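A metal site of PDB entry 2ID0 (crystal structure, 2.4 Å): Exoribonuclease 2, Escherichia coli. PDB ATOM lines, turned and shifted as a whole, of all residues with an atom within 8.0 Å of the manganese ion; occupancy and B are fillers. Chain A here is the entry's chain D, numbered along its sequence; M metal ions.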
ATOM      1  N   VAL A 198       2.794  13.936 -18.736  1.00  0.00           N
ATOM      2  CA  VAL A 198       3.870  14.186 -17.766  1.00  0.00           C
ATOM      3  C   VAL A 198       3.642  15.485 -16.985  1.00  0.00           C
ATOM      4  O   VAL A 198       2.753  16.265 -17.304  1.00  0.00           O
ATOM      5  CB  VAL A 198       5.260  14.167 -18.441  1.00  0.00           C
ATOM      6  CG1 VAL A 198       5.297  15.078 -19.680  1.00  0.00           C
ATOM      7  CG2 VAL A 198       6.324  14.570 -17.453  1.00  0.00           C
ATOM      8  N   THR A 199       4.448  15.715 -15.963  1.00  0.00           N
ATOM      9  CA  THR A 199       4.403  16.933 -15.217  1.00  0.00           C
ATOM     10  C   THR A 199       5.845  17.263 -14.935  1.00  0.00           C
ATOM     11  O   THR A 199       6.625  16.385 -14.594  1.00  0.00           O
ATOM     12  CB  THR A 199       3.675  16.751 -13.880  1.00  0.00           C
ATOM     13  OG1 THR A 199       4.128  15.535 -13.273  1.00  0.00           O
ATOM     14  CG2 THR A 199       2.151  16.685 -14.080  1.00  0.00           C
ATOM     15  N   ILE A 200       6.194  18.539 -15.112  1.00  0.00           N
ATOM     16  CA  ILE A 200       7.581  18.981 -14.995  1.00  0.00           C
ATOM     17  C   ILE A 200       7.571  20.188 -14.102  1.00  0.00           C
ATOM     18  O   ILE A 200       6.867  21.168 -14.357  1.00  0.00           O
ATOM     19  CB  ILE A 200       8.244  19.295 -16.371  1.00  0.00           C
ATOM     20  CG1 ILE A 200       8.259  18.043 -17.273  1.00  0.00           C
ATOM     21  CG2 ILE A 200       9.682  19.768 -16.171  1.00  0.00           C
ATOM     22  CD1 ILE A 200       8.096  18.328 -18.740  1.00  0.00           C
ATOM     23  N   ASP A 201       8.316  20.069 -13.005  1.00  0.00           N
ATOM     24  CA  ASP A 201       8.332  21.072 -11.943  1.00  0.00           C
ATOM     25  C   ASP A 201       9.652  20.908 -11.219  1.00  0.00           C
ATOM     26  O   ASP A 201      10.498  20.060 -11.588  1.00  0.00           O
ATOM     27  CB  ASP A 201       7.191  20.852 -10.937  1.00  0.00           C
ATOM     28  CG  ASP A 201       5.809  20.966 -11.569  1.00  0.00           C
ATOM     29  OD1 ASP A 201       5.383  22.093 -11.870  1.00  0.00           O
ATOM     30  OD2 ASP A 201       5.120  19.943 -11.741  1.00  0.00           O
ATOM     31  N   SER A 202       9.832  21.691 -10.172  1.00  0.00           N
ATOM     32  CA  SER A 202      10.979  21.600  -9.298  1.00  0.00           C
ATOM     33  C   SER A 202      11.007  20.299  -8.490  1.00  0.00           C
ATOM     34  O   SER A 202       9.960  19.641  -8.306  1.00  0.00           O
ATOM     35  CB  SER A 202      10.954  22.784  -8.347  1.00  0.00           C
ATOM     36  OG  SER A 202      12.244  23.349  -8.238  1.00  0.00           O
ATOM     37  N   THR A 205       8.760  20.344  -5.453  1.00  0.00           N
ATOM     38  CA  THR A 205       7.331  20.388  -5.814  1.00  0.00           C
ATOM     39  C   THR A 205       6.520  19.184  -5.382  1.00  0.00           C
ATOM     40  O   THR A 205       6.821  18.046  -5.777  1.00  0.00           O
ATOM     41  CB  THR A 205       7.109  20.686  -7.327  1.00  0.00           C
ATOM     42  OG1 THR A 205       7.460  22.060  -7.595  1.00  0.00           O
ATOM     43  CG2 THR A 205       5.651  20.446  -7.735  1.00  0.00           C
ATOM     44  N   ASP A 207       2.985  19.891  -5.361  1.00  0.00           N
ATOM     45  CA  ASP A 207       1.694  20.411  -5.837  1.00  0.00           C
ATOM     46  C   ASP A 207       1.644  20.416  -7.357  1.00  0.00           C
ATOM     47  O   ASP A 207       1.947  21.412  -7.986  1.00  0.00           O
ATOM     48  CB  ASP A 207       1.486  21.839  -5.317  1.00  0.00           C
ATOM     49  N   MET A 208       1.256  19.305  -7.962  1.00  0.00           N
ATOM     50  CA  MET A 208       1.201  19.225  -9.419  1.00  0.00           C
ATOM     51  C   MET A 208      -0.026  19.961  -9.958  1.00  0.00           C
ATOM     52  O   MET A 208      -1.144  19.507  -9.783  1.00  0.00           O
ATOM     53  CB  MET A 208       1.225  17.776  -9.894  1.00  0.00           C
ATOM     54  CG  MET A 208       2.622  17.157  -9.988  1.00  0.00           C
ATOM     55  SD  MET A 208       3.392  16.795  -8.227  1.00  0.00           S
ATOM     56  CE  MET A 208       2.418  15.142  -7.839  1.00  0.00           C
ATOM     57  N   ASP A 209       0.210  21.107 -10.601  1.00  0.00           N
ATOM     58  CA  ASP A 209      -0.847  21.998 -11.093  1.00  0.00           C
ATOM     59  C   ASP A 209      -1.209  21.778 -12.559  1.00  0.00           C
ATOM     60  O   ASP A 209      -2.372  21.937 -12.936  1.00  0.00           O
ATOM     61  CB  ASP A 209      -0.465  23.486 -10.873  1.00  0.00           C
ATOM     62  CG  ASP A 209       0.934  23.860 -11.425  1.00  0.00           C
ATOM     63  OD1 ASP A 209       1.953  23.233 -11.011  1.00  0.00           O
ATOM     64  OD2 ASP A 209       1.011  24.819 -12.252  1.00  0.00           O
ATOM     65  N   ASP A 210      -0.212  21.441 -13.373  1.00  0.00           N
ATOM     66  CA  ASP A 210      -0.365  21.303 -14.812  1.00  0.00           C
ATOM     67  C   ASP A 210       0.387  20.095 -15.359  1.00  0.00           C
ATOM     68  O   ASP A 210       1.399  19.659 -14.804  1.00  0.00           O
ATOM     69  CB  ASP A 210       0.141  22.547 -15.525  1.00  0.00           C
ATOM     70  CG  ASP A 210       1.617  22.785 -15.293  1.00  0.00           C
ATOM     71  OD1 ASP A 210       1.939  23.365 -14.246  1.00  0.00           O
ATOM     72  OD2 ASP A 210       2.443  22.386 -16.160  1.00  0.00           O
ATOM     73  N   ALA A 211      -0.138  19.579 -16.471  1.00  0.00           N
ATOM     74  CA  ALA A 211       0.435  18.438 -17.171  1.00  0.00           C
ATOM     75  C   ALA A 211       0.424  18.721 -18.663  1.00  0.00           C
ATOM     76  O   ALA A 211      -0.258  19.639 -19.113  1.00  0.00           O
ATOM     77  CB  ALA A 211      -0.334  17.176 -16.844  1.00  0.00           C
ATOM     78  N   LEU A 212       1.177  17.932 -19.422  1.00  0.00           N
ATOM     79  CA  LEU A 212       1.412  18.194 -20.829  1.00  0.00           C
ATOM     80  C   LEU A 212       1.497  16.941 -21.643  1.00  0.00           C
ATOM     81  O   LEU A 212       1.983  15.916 -21.160  1.00  0.00           O
ATOM     82  CB  LEU A 212       2.729  18.941 -21.013  1.00  0.00           C
ATOM     83  CG  LEU A 212       3.054  20.105 -20.081  1.00  0.00           C
ATOM     84  CD1 LEU A 212       4.481  20.521 -20.316  1.00  0.00           C
ATOM     85  CD2 LEU A 212       2.083  21.251 -20.327  1.00  0.00           C
ATOM     86  N   ALA A 227      -3.209  20.321 -19.395  1.00  0.00           N
ATOM     87  CA  ALA A 227      -4.228  19.884 -18.476  1.00  0.00           C
ATOM     88  C   ALA A 227      -3.930  20.468 -17.112  1.00  0.00           C
ATOM     89  O   ALA A 227      -2.899  20.169 -16.510  1.00  0.00           O
ATOM     90  CB  ALA A 227      -4.297  18.350 -18.434  1.00  0.00           C
ATOM     91  N   ILE A 228      -4.832  21.323 -16.668  1.00  0.00           N
ATOM     92  CA  ILE A 228      -4.683  21.989 -15.394  1.00  0.00           C
ATOM     93  C   ILE A 228      -5.649  21.389 -14.405  1.00  0.00           C
ATOM     94  O   ILE A 228      -6.785  21.051 -14.751  1.00  0.00           O
ATOM     95  CB  ILE A 228      -4.951  23.533 -15.480  1.00  0.00           C
ATOM     96  CG1 ILE A 228      -4.072  24.204 -16.542  1.00  0.00           C
ATOM     97  CG2 ILE A 228      -4.731  24.194 -14.131  1.00  0.00           C
ATOM     98  CD1 ILE A 228      -2.598  23.834 -16.514  1.00  0.00           C
ATOM     99  N   LEU A 273      -1.534  16.564  -9.505  1.00  0.00           N
ATOM    100  CA  LEU A 273      -1.499  15.668 -10.649  1.00  0.00           C
ATOM    101  C   LEU A 273      -0.433  14.579 -10.459  1.00  0.00           C
ATOM    102  O   LEU A 273       0.601  14.538 -11.153  1.00  0.00           O
ATOM    103  CB  LEU A 273      -1.289  16.440 -11.943  1.00  0.00           C
ATOM    104  CG  LEU A 273      -2.257  17.587 -12.218  1.00  0.00           C
ATOM    105  CD1 LEU A 273      -1.759  18.290 -13.439  1.00  0.00           C
ATOM    106  CD2 LEU A 273      -3.744  17.160 -12.385  1.00  0.00           C
ATOM    107  N   TYR A 313      12.975  19.654 -13.455  1.00  0.00           N
ATOM    108  CA  TYR A 313      13.641  20.642 -14.306  1.00  0.00           C
ATOM    109  C   TYR A 313      15.086  20.324 -14.668  1.00  0.00           C
ATOM    110  O   TYR A 313      15.389  20.065 -15.834  1.00  0.00           O
ATOM    111  CB  TYR A 313      13.546  22.023 -13.659  1.00  0.00           C
ATOM    112  CG  TYR A 313      12.188  22.661 -13.806  1.00  0.00           C
ATOM    113  CD1 TYR A 313      11.718  23.572 -12.863  1.00  0.00           C
ATOM    114  CD2 TYR A 313      11.391  22.369 -14.890  1.00  0.00           C
ATOM    115  CE1 TYR A 313      10.471  24.164 -13.017  1.00  0.00           C
ATOM    116  CE2 TYR A 313      10.149  22.931 -15.041  1.00  0.00           C
ATOM    117  CZ  TYR A 313       9.686  23.825 -14.115  1.00  0.00           C
ATOM    118  OH  TYR A 313       8.425  24.355 -14.310  1.00  0.00           O
ATOM    119  N   VAL A 389       7.971  24.188 -20.018  1.00  0.00           N
ATOM    120  CA  VAL A 389       6.747  24.457 -19.260  1.00  0.00           C
ATOM    121  C   VAL A 389       6.208  25.878 -19.565  1.00  0.00           C
ATOM    122  O   VAL A 389       5.036  26.021 -19.930  1.00  0.00           O
ATOM    123  CB  VAL A 389       6.957  24.207 -17.733  1.00  0.00           C
ATOM    124  CG1 VAL A 389       5.746  24.654 -16.903  1.00  0.00           C
ATOM    125  CG2 VAL A 389       7.222  22.744 -17.487  1.00  0.00           C
ATOM    126  N   MET A 393       2.544  27.105 -21.053  1.00  0.00           N
ATOM    127  CA  MET A 393       1.704  27.939 -20.174  1.00  0.00           C
ATOM    128  C   MET A 393       1.176  29.219 -20.836  1.00  0.00           C
ATOM    129  O   MET A 393      -0.029  29.538 -20.738  1.00  0.00           O
ATOM    130  CB  MET A 393       2.475  28.310 -18.908  1.00  0.00           C
ATOM    131  CG  MET A 393       2.912  27.133 -18.040  1.00  0.00           C
ATOM    132  SD  MET A 393       1.473  25.853 -17.648  1.00  0.00           S
ATOM    133  CE  MET A 393       1.953  24.398 -18.859  1.00  0.00           C
ATOM    134  N   THR A 496      -4.066  28.802 -15.642  1.00  0.00           N
ATOM    135  CA  THR A 496      -3.065  27.762 -15.486  1.00  0.00           C
ATOM    136  C   THR A 496      -2.587  27.592 -14.023  1.00  0.00           C
ATOM    137  O   THR A 496      -1.792  26.672 -13.713  1.00  0.00           O
ATOM    138  CB  THR A 496      -1.880  28.026 -16.473  1.00  0.00           C
ATOM    139  OG1 THR A 496      -2.380  28.069 -17.809  1.00  0.00           O
ATOM    140  CG2 THR A 496      -0.849  26.963 -16.419  1.00  0.00           C
ATOM    141  N   SER A 497      -3.086  28.441 -13.122  1.00  0.00           N
ATOM    142  CA  SER A 497      -2.653  28.388 -11.699  1.00  0.00           C
ATOM    143  C   SER A 497      -3.759  28.806 -10.726  1.00  0.00           C
ATOM    144  O   SER A 497      -3.553  29.774  -9.957  1.00  0.00           O
ATOM    145  CB  SER A 497      -1.392  29.240 -11.452  1.00  0.00           C
ATOM    146  OG  SER A 497      -0.425  29.079 -12.494  1.00  0.00           O
ATOM    147  N   ILE A 499      -4.800  27.207  -8.243  1.00  0.00           N
ATOM    148  CA  ILE A 499      -4.390  26.794  -6.910  1.00  0.00           C
ATOM    149  C   ILE A 499      -3.701  27.982  -6.195  1.00  0.00           C
ATOM    150  O   ILE A 499      -3.771  28.088  -4.971  1.00  0.00           O
ATOM    151  CB  ILE A 499      -3.446  25.572  -7.029  1.00  0.00           C
ATOM    152  CG1 ILE A 499      -4.157  24.463  -7.837  1.00  0.00           C
ATOM    153  CG2 ILE A 499      -3.020  25.070  -5.637  1.00  0.00           C
ATOM    154  CD1 ILE A 499      -3.290  23.763  -8.889  1.00  0.00           C
ATOM    155  N   ARG A 500      -3.045  28.850  -6.957  1.00  0.00           N
ATOM    156  CA  ARG A 500      -2.419  30.004  -6.340  1.00  0.00           C
ATOM    157  C   ARG A 500      -2.973  31.357  -6.767  1.00  0.00           C
ATOM    158  O   ARG A 500      -2.683  32.331  -6.127  1.00  0.00           O
ATOM    159  CB  ARG A 500      -0.903  29.947  -6.511  1.00  0.00           C
ATOM    160  CG  ARG A 500      -0.421  29.617  -7.886  1.00  0.00           C
ATOM    161  CD  ARG A 500       1.048  29.862  -8.013  1.00  0.00           C
ATOM    162  NE  ARG A 500       1.456  29.777  -9.403  1.00  0.00           N
ATOM    163  CZ  ARG A 500       2.599  29.242  -9.818  1.00  0.00           C
ATOM    164  NH1 ARG A 500       3.467  28.755  -8.924  1.00  0.00           N
ATOM    165  NH2 ARG A 500       2.867  29.184 -11.131  1.00  0.00           N
HETATM  166 MN    MN M   1       3.556  22.640 -12.745  1.00  0.00          MN
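The manganese ion is bound by the side-chain carboxylate of Asp 201, the side-chain carboxylate of Asp 210 and the side-chain carboxylate of Asp 209.
O of Asp 201 is in hydrogen-bond range of N of Tyr 313 (3.1 Å).
Ile 200 touches the manganese ion.
Of the 22 residues printed, 4 come within 4 Å of the manganese ion.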
